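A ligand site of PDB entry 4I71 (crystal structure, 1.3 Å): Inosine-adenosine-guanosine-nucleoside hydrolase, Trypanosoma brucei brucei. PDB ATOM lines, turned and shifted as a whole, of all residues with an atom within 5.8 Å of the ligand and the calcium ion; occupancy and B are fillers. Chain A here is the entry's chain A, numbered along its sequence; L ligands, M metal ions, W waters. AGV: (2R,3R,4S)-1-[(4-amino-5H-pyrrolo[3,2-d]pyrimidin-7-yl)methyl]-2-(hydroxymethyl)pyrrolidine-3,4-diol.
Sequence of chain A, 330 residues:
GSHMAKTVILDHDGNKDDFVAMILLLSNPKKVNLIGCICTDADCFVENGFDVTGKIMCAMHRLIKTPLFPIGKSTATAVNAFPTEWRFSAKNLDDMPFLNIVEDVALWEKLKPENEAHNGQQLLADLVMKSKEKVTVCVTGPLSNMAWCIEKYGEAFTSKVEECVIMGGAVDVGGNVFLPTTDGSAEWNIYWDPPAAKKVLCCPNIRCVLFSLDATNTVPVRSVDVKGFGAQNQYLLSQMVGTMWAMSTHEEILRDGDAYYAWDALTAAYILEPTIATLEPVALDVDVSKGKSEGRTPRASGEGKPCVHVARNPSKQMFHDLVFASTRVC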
ATOM      1  N   HIS A  12      28.783 -15.712 -33.157  1.00  0.00           N
ATOM      2  CA  HIS A  12      27.409 -16.162 -33.129  1.00  0.00           C
ATOM      3  C   HIS A  12      27.277 -17.651 -33.202  1.00  0.00           C
ATOM      4  O   HIS A  12      28.260 -18.355 -33.476  1.00  0.00           O
ATOM      5  CB  HIS A  12      26.608 -15.504 -34.223  1.00  0.00           C
ATOM      6  CG  HIS A  12      26.856 -16.008 -35.595  1.00  0.00           C
ATOM      7  ND1 HIS A  12      26.218 -17.133 -36.076  1.00  0.00           N
ATOM      8  CD2 HIS A  12      27.634 -15.532 -36.594  1.00  0.00           C
ATOM      9  CE1 HIS A  12      26.623 -17.335 -37.320  1.00  0.00           C
ATOM     10  NE2 HIS A  12      27.471 -16.384 -37.669  1.00  0.00           N
ATOM     11  N   ASP A  13      26.071 -18.156 -32.941  1.00  0.00           N
ATOM     12  CA  ASP A  13      25.815 -19.591 -33.045  1.00  0.00           C
ATOM     13  C   ASP A  13      24.644 -19.950 -33.910  1.00  0.00           C
ATOM     14  O   ASP A  13      24.042 -21.007 -33.735  1.00  0.00           O
ATOM     15  CB  ASP A  13      25.686 -20.204 -31.669  1.00  0.00           C
ATOM     16  CG  ASP A  13      24.458 -19.799 -30.920  1.00  0.00           C
ATOM     17  OD1 ASP A  13      23.895 -18.715 -31.232  1.00  0.00           O
ATOM     18  OD2 ASP A  13      24.061 -20.600 -29.993  1.00  0.00           O
ATOM     19  N   GLY A  14      24.335 -19.096 -34.896  1.00  0.00           N
ATOM     20  CA  GLY A  14      23.609 -19.568 -36.080  1.00  0.00           C
ATOM     21  C   GLY A  14      22.139 -19.907 -35.939  1.00  0.00           C
ATOM     22  O   GLY A  14      21.652 -20.660 -36.787  1.00  0.00           O
ATOM     23  N   ASN A  15      21.451 -19.398 -34.920  1.00  0.00           N
ATOM     24  CA  ASN A  15      20.010 -19.501 -34.931  1.00  0.00           C
ATOM     25  C   ASN A  15      19.423 -18.317 -35.766  1.00  0.00           C
ATOM     26  O   ASN A  15      20.156 -17.439 -36.239  1.00  0.00           O
ATOM     27  CB  ASN A  15      19.413 -19.570 -33.527  1.00  0.00           C
ATOM     28  CG  ASN A  15      18.199 -20.529 -33.497  1.00  0.00           C
ATOM     29  OD1 ASN A  15      17.062 -20.072 -33.541  1.00  0.00           O
ATOM     30  ND2 ASN A  15      18.434 -21.818 -33.484  1.00  0.00           N
ATOM     31  N   LYS A  16      18.108 -18.327 -35.962  1.00  0.00           N
ATOM     32  CA  LYS A  16      17.486 -17.300 -36.777  1.00  0.00           C
ATOM     33  C   LYS A  16      17.823 -15.918 -36.288  1.00  0.00           C
ATOM     34  O   LYS A  16      18.167 -15.014 -37.079  1.00  0.00           O
ATOM     35  CB  LYS A  16      15.952 -17.529 -36.798  1.00  0.00           C
ATOM     36  CG  LYS A  16      15.555 -18.831 -37.527  1.00  0.00           C
ATOM     37  CD  LYS A  16      14.186 -19.371 -37.073  1.00  0.00           C
ATOM     38  CE  LYS A  16      14.302 -19.897 -35.639  1.00  0.00           C
ATOM     39  NZ  LYS A  16      12.966 -20.454 -35.224  1.00  0.00           N
ATOM     40  N   ASP A  17      17.746 -15.756 -34.982  1.00  0.00           N
ATOM     41  CA  ASP A  17      17.996 -14.527 -34.302  1.00  0.00           C
ATOM     42  C   ASP A  17      19.445 -14.003 -34.551  1.00  0.00           C
ATOM     43  O   ASP A  17      19.713 -12.833 -34.713  1.00  0.00           O
ATOM     44  CB  ASP A  17      17.728 -14.817 -32.820  1.00  0.00           C
ATOM     45  CG  ASP A  17      17.885 -13.643 -31.919  1.00  0.00           C
ATOM     46  OD1 ASP A  17      17.585 -12.464 -32.297  1.00  0.00           O
ATOM     47  OD2 ASP A  17      18.296 -13.931 -30.755  1.00  0.00           O
ATOM     48  N   ASP A  18      20.375 -14.933 -34.535  1.00  0.00           N
ATOM     49  CA  ASP A  18      21.812 -14.620 -34.821  1.00  0.00           C
ATOM     50  C   ASP A  18      21.965 -13.946 -36.196  1.00  0.00           C
ATOM     51  O   ASP A  18      22.746 -13.010 -36.364  1.00  0.00           O
ATOM     52  CB  ASP A  18      22.693 -15.868 -34.752  1.00  0.00           C
ATOM     53  CG  ASP A  18      22.733 -16.469 -33.376  1.00  0.00           C
ATOM     54  OD1 ASP A  18      23.689 -16.142 -32.612  1.00  0.00           O
ATOM     55  OD2 ASP A  18      21.803 -17.247 -33.020  1.00  0.00           O
ATOM     56  N   ASP A  43      23.702 -23.391 -31.044  1.00  0.00           N
ATOM     57  CA  ASP A  43      22.277 -23.397 -31.497  1.00  0.00           C
ATOM     58  C   ASP A  43      22.127 -23.560 -32.997  1.00  0.00           C
ATOM     59  O   ASP A  43      21.146 -23.060 -33.597  1.00  0.00           O
ATOM     60  CB  ASP A  43      21.577 -22.134 -30.982  1.00  0.00           C
ATOM     61  CG  ASP A  43      20.096 -22.259 -30.751  1.00  0.00           C
ATOM     62  OD1 ASP A  43      19.542 -23.366 -30.787  1.00  0.00           O
ATOM     63  OD2 ASP A  43      19.479 -21.175 -30.500  1.00  0.00           O
ATOM     64  N   PHE A  82      22.407 -27.795 -27.069  1.00  0.00           N
ATOM     65  CA  PHE A  82      21.091 -27.312 -27.384  1.00  0.00           C
ATOM     66  C   PHE A  82      20.175 -28.413 -27.818  1.00  0.00           C
ATOM     67  O   PHE A  82      20.611 -29.435 -28.336  1.00  0.00           O
ATOM     68  CB  PHE A  82      21.134 -26.227 -28.484  1.00  0.00           C
ATOM     69  CG  PHE A  82      21.427 -24.832 -27.961  1.00  0.00           C
ATOM     70  CD1 PHE A  82      20.382 -24.059 -27.463  1.00  0.00           C
ATOM     71  CD2 PHE A  82      22.698 -24.317 -27.931  1.00  0.00           C
ATOM     72  CE1 PHE A  82      20.579 -22.834 -26.976  1.00  0.00           C
ATOM     73  CE2 PHE A  82      22.916 -23.053 -27.435  1.00  0.00           C
ATOM     74  CZ  PHE A  82      21.864 -22.302 -26.956  1.00  0.00           C
ATOM     75  N   TRP A  86      15.957 -27.194 -32.271  1.00  0.00           N
ATOM     76  CA  TRP A  86      16.316 -25.775 -32.422  1.00  0.00           C
ATOM     77  C   TRP A  86      17.506 -25.592 -33.369  1.00  0.00           C
ATOM     78  O   TRP A  86      17.619 -24.601 -34.094  1.00  0.00           O
ATOM     79  CB  TRP A  86      16.650 -25.151 -31.092  1.00  0.00           C
ATOM     80  CG  TRP A  86      15.462 -25.015 -30.148  1.00  0.00           C
ATOM     81  CD1 TRP A  86      14.144 -25.275 -30.401  1.00  0.00           C
ATOM     82  CD2 TRP A  86      15.530 -24.556 -28.812  1.00  0.00           C
ATOM     83  NE1 TRP A  86      13.408 -25.016 -29.283  1.00  0.00           N
ATOM     84  CE2 TRP A  86      14.230 -24.575 -28.288  1.00  0.00           C
ATOM     85  CE3 TRP A  86      16.579 -24.123 -28.001  1.00  0.00           C
ATOM     86  CZ2 TRP A  86      13.951 -24.177 -26.970  1.00  0.00           C
ATOM     87  CZ3 TRP A  86      16.297 -23.732 -26.689  1.00  0.00           C
ATOM     88  CH2 TRP A  86      15.007 -23.778 -26.201  1.00  0.00           C
ATOM     89  N   THR A 140      26.697 -13.484 -29.530  1.00  0.00           N
ATOM     90  CA  THR A 140      25.302 -13.869 -29.552  1.00  0.00           C
ATOM     91  C   THR A 140      25.101 -15.366 -29.388  1.00  0.00           C
ATOM     92  O   THR A 140      23.978 -15.870 -29.409  1.00  0.00           O
ATOM     93  CB  THR A 140      24.607 -13.348 -30.794  1.00  0.00           C
ATOM     94  OG1 THR A 140      25.245 -13.917 -31.961  1.00  0.00           O
ATOM     95  CG2 THR A 140      24.674 -11.849 -30.864  1.00  0.00           C
ATOM     96  N   GLY A 141      26.174 -16.118 -29.207  1.00  0.00           N
ATOM     97  CA  GLY A 141      26.137 -17.484 -28.770  1.00  0.00           C
ATOM     98  C   GLY A 141      26.849 -17.629 -27.429  1.00  0.00           C
ATOM     99  O   GLY A 141      27.057 -16.636 -26.718  1.00  0.00           O
ATOM    100  N   MET A 167      24.777 -11.387 -25.522  1.00  0.00           N
ATOM    101  CA  MET A 167      23.431 -11.924 -25.236  1.00  0.00           C
ATOM    102  C   MET A 167      23.630 -13.123 -24.331  1.00  0.00           C
ATOM    103  O   MET A 167      24.210 -14.117 -24.732  1.00  0.00           O
ATOM    104  CB  MET A 167      22.708 -12.252 -26.521  1.00  0.00           C
ATOM    105  CG  MET A 167      21.230 -12.444 -26.294  1.00  0.00           C
ATOM    106  SD  MET A 167      20.815 -14.020 -25.464  1.00  0.00           S
ATOM    107  CE  MET A 167      19.797 -13.481 -24.029  1.00  0.00           C
ATOM    108  N   ASN A 176      15.445 -19.570 -19.245  1.00  0.00           N
ATOM    109  CA  ASN A 176      14.752 -20.203 -20.353  1.00  0.00           C
ATOM    110  C   ASN A 176      15.181 -21.644 -20.597  1.00  0.00           C
ATOM    111  O   ASN A 176      14.767 -22.224 -21.620  1.00  0.00           O
ATOM    112  CB  ASN A 176      14.781 -19.317 -21.611  1.00  0.00           C
ATOM    113  CG  ASN A 176      16.138 -19.114 -22.208  1.00  0.00           C
ATOM    114  OD1 ASN A 176      17.104 -19.802 -21.811  1.00  0.00           O
ATOM    115  ND2 ASN A 176      16.223 -18.204 -23.203  1.00  0.00           N
ATOM    116  N   GLU A 187      19.777 -19.258 -18.379  1.00  0.00           N
ATOM    117  CA  GLU A 187      19.589 -18.917 -19.794  1.00  0.00           C
ATOM    118  C   GLU A 187      20.534 -19.776 -20.640  1.00  0.00           C
ATOM    119  O   GLU A 187      21.603 -20.135 -20.201  1.00  0.00           O
ATOM    120  CB  GLU A 187      19.771 -17.402 -19.971  1.00  0.00           C
ATOM    121  CG  GLU A 187      19.669 -16.877 -21.379  1.00  0.00           C
ATOM    122  CD  GLU A 187      20.886 -17.188 -22.245  1.00  0.00           C
ATOM    123  OE1 GLU A 187      22.025 -17.212 -21.698  1.00  0.00           O
ATOM    124  OE2 GLU A 187      20.717 -17.407 -23.504  1.00  0.00           O
ATOM    125  N   TRP A 188      20.082 -20.130 -21.842  1.00  0.00           N
ATOM    126  CA  TRP A 188      20.712 -21.155 -22.662  1.00  0.00           C
ATOM    127  C   TRP A 188      22.173 -20.864 -23.056  1.00  0.00           C
ATOM    128  O   TRP A 188      23.016 -21.773 -23.030  1.00  0.00           O
ATOM    129  CB  TRP A 188      19.856 -21.437 -23.933  1.00  0.00           C
ATOM    130  CG  TRP A 188      18.935 -22.587 -23.736  1.00  0.00           C
ATOM    131  CD1 TRP A 188      17.588 -22.582 -23.500  1.00  0.00           C
ATOM    132  CD2 TRP A 188      19.345 -23.954 -23.746  1.00  0.00           C
ATOM    133  NE1 TRP A 188      17.146 -23.861 -23.369  1.00  0.00           N
ATOM    134  CE2 TRP A 188      18.198 -24.728 -23.499  1.00  0.00           C
ATOM    135  CE3 TRP A 188      20.573 -24.587 -23.911  1.00  0.00           C
ATOM    136  CZ2 TRP A 188      18.251 -26.116 -23.429  1.00  0.00           C
ATOM    137  CZ3 TRP A 188      20.631 -25.986 -23.863  1.00  0.00           C
ATOM    138  CH2 TRP A 188      19.474 -26.714 -23.617  1.00  0.00           C
ATOM    139  N   ASN A 189      22.487 -19.646 -23.475  1.00  0.00           N
ATOM    140  CA  ASN A 189      23.842 -19.349 -23.914  1.00  0.00           C
ATOM    141  C   ASN A 189      24.858 -19.588 -22.798  1.00  0.00           C
ATOM    142  O   ASN A 189      25.970 -20.063 -23.036  1.00  0.00           O
ATOM    143  CB  ASN A 189      24.005 -17.924 -24.448  1.00  0.00           C
ATOM    144  CG  ASN A 189      23.376 -17.733 -25.794  1.00  0.00           C
ATOM    145  OD1 ASN A 189      22.992 -18.705 -26.464  1.00  0.00           O
ATOM    146  ND2 ASN A 189      23.249 -16.465 -26.198  1.00  0.00           N
ATOM    147  N   LEU A 213      17.976 -11.875 -20.142  1.00  0.00           N
ATOM    148  CA  LEU A 213      16.541 -12.014 -20.394  1.00  0.00           C
ATOM    149  C   LEU A 213      15.762 -10.827 -19.779  1.00  0.00           C
ATOM    150  O   LEU A 213      14.674 -10.488 -20.250  1.00  0.00           O
ATOM    151  CB  LEU A 213      16.006 -13.360 -19.934  1.00  0.00           C
ATOM    152  CG  LEU A 213      16.632 -14.623 -20.561  1.00  0.00           C
ATOM    153  CD1 LEU A 213      15.907 -15.866 -20.069  1.00  0.00           C
ATOM    154  CD2 LEU A 213      16.660 -14.507 -22.069  1.00  0.00           C
ATOM    155  N   GLU A 251       5.796 -19.616 -31.448  1.00  0.00           N
ATOM    156  CA  GLU A 251       6.382 -20.225 -30.252  1.00  0.00           C
ATOM    157  C   GLU A 251       5.762 -19.674 -28.979  1.00  0.00           C
ATOM    158  O   GLU A 251       5.632 -20.377 -27.997  1.00  0.00           O
ATOM    159  CB  GLU A 251       7.900 -20.064 -30.225  1.00  0.00           C
ATOM    160  CG  GLU A 251       8.539 -20.845 -31.401  1.00  0.00           C
ATOM    161  CD  GLU A 251      10.036 -21.005 -31.347  1.00  0.00           C
ATOM    162  OE1 GLU A 251      10.612 -20.919 -30.231  1.00  0.00           O
ATOM    163  OE2 GLU A 251      10.642 -21.211 -32.444  1.00  0.00           O
ATOM    164  N   ARG A 255       4.313 -22.350 -26.351  1.00  0.00           N
ATOM    165  CA  ARG A 255       4.891 -22.407 -25.012  1.00  0.00           C
ATOM    166  C   ARG A 255       4.224 -21.439 -24.021  1.00  0.00           C
ATOM    167  O   ARG A 255       4.830 -21.030 -23.048  1.00  0.00           O
ATOM    168  CB  ARG A 255       6.398 -22.207 -25.072  1.00  0.00           C
ATOM    169  CG  ARG A 255       7.125 -23.311 -25.778  1.00  0.00           C
ATOM    170  CD  ARG A 255       8.692 -23.278 -25.407  1.00  0.00           C
ATOM    171  NE  ARG A 255       9.237 -22.009 -25.893  1.00  0.00           N
ATOM    172  CZ  ARG A 255       9.681 -21.790 -27.130  1.00  0.00           C
ATOM    173  NH1 ARG A 255       9.709 -22.744 -28.036  1.00  0.00           N
ATOM    174  NH2 ARG A 255      10.085 -20.547 -27.440  1.00  0.00           N
ATOM    175  N   ALA A 259       8.072 -17.012 -25.391  1.00  0.00           N
ATOM    176  CA  ALA A 259       8.202 -16.686 -26.802  1.00  0.00           C
ATOM    177  C   ALA A 259       9.591 -17.006 -27.396  1.00  0.00           C
ATOM    178  O   ALA A 259      10.547 -17.265 -26.686  1.00  0.00           O
ATOM    179  CB  ALA A 259       7.901 -15.194 -27.004  1.00  0.00           C
ATOM    180  N   TYR A 260       9.637 -16.950 -28.704  1.00  0.00           N
ATOM    181  CA  TYR A 260      10.918 -16.678 -29.382  1.00  0.00           C
ATOM    182  C   TYR A 260      11.052 -15.169 -29.331  1.00  0.00           C
ATOM    183  O   TYR A 260      10.123 -14.434 -29.672  1.00  0.00           O
ATOM    184  CB  TYR A 260      10.884 -17.261 -30.808  1.00  0.00           C
ATOM    185  CG  TYR A 260      12.249 -17.335 -31.484  1.00  0.00           C
ATOM    186  CD1 TYR A 260      12.952 -18.544 -31.518  1.00  0.00           C
ATOM    187  CD2 TYR A 260      12.823 -16.248 -32.071  1.00  0.00           C
ATOM    188  CE1 TYR A 260      14.204 -18.646 -32.136  1.00  0.00           C
ATOM    189  CE2 TYR A 260      14.099 -16.328 -32.707  1.00  0.00           C
ATOM    190  CZ  TYR A 260      14.781 -17.552 -32.716  1.00  0.00           C
ATOM    191  OH  TYR A 260      16.023 -17.601 -33.343  1.00  0.00           O
ATOM    192  N   TRP A 263      16.359 -11.753 -29.161  1.00  0.00           N
ATOM    193  CA  TRP A 263      17.428 -11.709 -28.167  1.00  0.00           C
ATOM    194  C   TRP A 263      18.707 -11.101 -28.742  1.00  0.00           C
ATOM    195  O   TRP A 263      19.241 -10.081 -28.229  1.00  0.00           O
ATOM    196  CB  TRP A 263      17.716 -13.055 -27.643  1.00  0.00           C
ATOM    197  CG  TRP A 263      16.728 -13.943 -27.017  1.00  0.00           C
ATOM    198  CD1 TRP A 263      16.339 -13.958 -25.720  1.00  0.00           C
ATOM    199  CD2 TRP A 263      16.034 -15.066 -27.634  1.00  0.00           C
ATOM    200  NE1 TRP A 263      15.457 -15.005 -25.484  1.00  0.00           N
ATOM    201  CE2 TRP A 263      15.252 -15.693 -26.633  1.00  0.00           C
ATOM    202  CE3 TRP A 263      15.990 -15.565 -28.949  1.00  0.00           C
ATOM    203  CZ2 TRP A 263      14.476 -16.811 -26.884  1.00  0.00           C
ATOM    204  CZ3 TRP A 263      15.223 -16.691 -29.193  1.00  0.00           C
ATOM    205  CH2 TRP A 263      14.470 -17.288 -28.177  1.00  0.00           C
ATOM    206  N   ASP A 264      19.232 -11.727 -29.771  1.00  0.00           N
ATOM    207  CA  ASP A 264      20.481 -11.324 -30.366  1.00  0.00           C
ATOM    208  C   ASP A 264      20.344 -10.074 -31.196  1.00  0.00           C
ATOM    209  O   ASP A 264      21.284  -9.247 -31.285  1.00  0.00           O
ATOM    210  CB  ASP A 264      21.013 -12.471 -31.260  1.00  0.00           C
ATOM    211  CG  ASP A 264      21.306 -13.764 -30.518  1.00  0.00           C
ATOM    212  OD1 ASP A 264      21.328 -13.723 -29.267  1.00  0.00           O
ATOM    213  OD2 ASP A 264      21.453 -14.786 -31.222  1.00  0.00           O
HETATM  214  O5' AGV L   1      18.673 -18.065 -25.009  1.00  0.00           O
HETATM  215  C5' AGV L   1      18.639 -17.230 -26.171  1.00  0.00           C
HETATM  216  C4' AGV L   1      19.706 -17.522 -27.219  1.00  0.00           C
HETATM  217  C3' AGV L   1      19.880 -16.395 -28.244  1.00  0.00           C
HETATM  218  O3' AGV L   1      21.263 -16.142 -28.520  1.00  0.00           O
HETATM  219  N4' AGV L   1      19.422 -18.716 -28.096  1.00  0.00           N
HETATM  220  C1' AGV L   1      18.555 -18.197 -29.210  1.00  0.00           C
HETATM  221  C2' AGV L   1      19.117 -16.864 -29.495  1.00  0.00           C
HETATM  222  O2' AGV L   1      19.956 -16.969 -30.669  1.00  0.00           O
HETATM  223  C7  AGV L   1      18.995 -20.048 -27.429  1.00  0.00           C
HETATM  224  C9  AGV L   1      17.515 -20.273 -27.442  1.00  0.00           C
HETATM  225  C8  AGV L   1      16.691 -20.063 -26.362  1.00  0.00           C
HETATM  226  N7  AGV L   1      15.423 -20.366 -26.725  1.00  0.00           N
HETATM  227  C5  AGV L   1      15.380 -20.770 -28.039  1.00  0.00           C
HETATM  228  C4  AGV L   1      16.696 -20.720 -28.495  1.00  0.00           C
HETATM  229  C6  AGV L   1      14.339 -21.158 -28.889  1.00  0.00           C
HETATM  230  N6  AGV L   1      13.051 -21.178 -28.524  1.00  0.00           N
HETATM  231  N1  AGV L   1      14.676 -21.506 -30.160  1.00  0.00           N
HETATM  232  C2  AGV L   1      15.949 -21.461 -30.517  1.00  0.00           C
HETATM  233  N3  AGV L   1      16.987 -21.094 -29.751  1.00  0.00           N
HETATM  234 CA    CA M   1      22.385 -17.028 -30.627  1.00  0.00          CA
HETATM  235  O   HOH W   1      22.113 -18.941 -28.990  1.00  0.00           O
HETATM  236  O   HOH W   2      12.929 -20.539 -25.533  1.00  0.00           O
HETATM  237  O   HOH W   3      13.104 -21.975 -32.474  1.00  0.00           O
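The side-chain carboxylate (OD2) of Asp 43 is in salt-bridge range of a nitrogen (N4') of the ligand. The side-chain carboxylate of Glu 187 lies within hydrogen-bond range of an oxygen (O5') of the ligand (2.6 Å). A nitrogen (N6) of the ligand lies within hydrogen-bond range of the side-chain carboxylate (OE1) of Glu 251 (3.0 Å). An oxygen (O5') of the ligand sits at hydrogen-bond distance from the side-chain amide nitrogen (ND2) of Asn 176. O3' of the ligand sits close to ND2 of Asn 189 (3.1 Å). The side-chain carboxylate (OD2) of Asp 17 sits close to an oxygen (O2') of the ligand, at 3.5 Å. O3' of the ligand lies close to SD of Met 167.
ND2 of Asn 189 lies close to O of Thr 140, 3.3 Å away. The side-chain carboxylate (OD2) of Asp 13 is in hydrogen-bond range of the backbone NH (N) of Asp 43 (3.0 Å). The backbone NH (N) of Asn 15 sits close to the side-chain carboxylate (OD2) of Asp 18, 2.9 Å away. N of Asp 264 is in hydrogen-bond range of OD2 of Asp 17 (2.6 Å). The backbone NH (N) of Asn 189 sits at hydrogen-bond distance from the side-chain carboxylate (OE2) of Glu 187. The backbone carbonyl oxygen (O) of Met 167 is in hydrogen-bond range of the side-chain amide nitrogen (ND2) of Asn 189 (2.9 Å). The backbone carbonyl oxygen (O) of Trp 86 is in hydrogen-bond range of the side-chain amide nitrogen (ND2) of Asn 15 (3.0 Å). The backbone NH (N) of Lys 16 is in hydrogen-bond range of the side-chain hydroxyl (OH) of Tyr 260, at 3.4 Å.
N6 of the ligand sits close to NH2 of Arg 255. Asn 15 touches the ligand (OD1 to C2, 3.5 Å). Phe 82 touches the ligand (CE1 to C7, 3.2 Å). Trp 86 touches the ligand. CB of Trp 188 touches O5' of the ligand, 3.7 Å away. Tyr 260 touches the ligand. Trp 263 touches the ligand. Hydrophobic or aromatic side chains that line the ligand: Phe 82, Trp 86, Met 167, Trp 188, Tyr 260 and Trp 263. 17 residues have an atom within 4 Å of the ligand: Asn 15, Asp 17, Asp 18, Asp 43, Phe 82, Trp 86, Thr 140, Met 167, Asn 176, Glu 187, Trp 188, Asn 189, Glu 251, Arg 255, Tyr 260, Trp 263 and Asp 264.
The nearest printed residue that does not touch the calcium ion is Gly 141 (4.1 Å).
O of Thr 140 binds the calcium ion, 2.3 Å away. The calcium ion is bound by the side-chain carboxylate (OD1) of Asp 13 (2.3 Å). An oxygen (O2') of the ligand binds the calcium ion (2.4 Å). OD2 of Asp 18 binds the calcium ion (2.5 Å). The side-chain carboxylate (OD2) of Asp 264 is bound to the calcium ion. The calcium ion is bound by water W1 (2.5 Å). The calcium ion is bound by the side-chain carboxylate (OD1) of Asp 18. The calcium ion is bound by O3' of the ligand, at 2.5 Å. The calcium ion has eight donor atoms within binding distance.
Water W1 bridges the side-chain amide oxygen of Asn 189 (2.7 Å) and the side-chain carboxylate of Asp 13 (2.7 Å). Water W2 bridges a nitrogen (N7) of the ligand (2.8 Å) and the guanidinium group of Arg 255 (3.4 Å). Water W3 lies within hydrogen-bond range of OE2 of Glu 251 (2.6 Å), N1 of the ligand (2.8 Å) and NZ of Lys 16 (3.1 Å).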
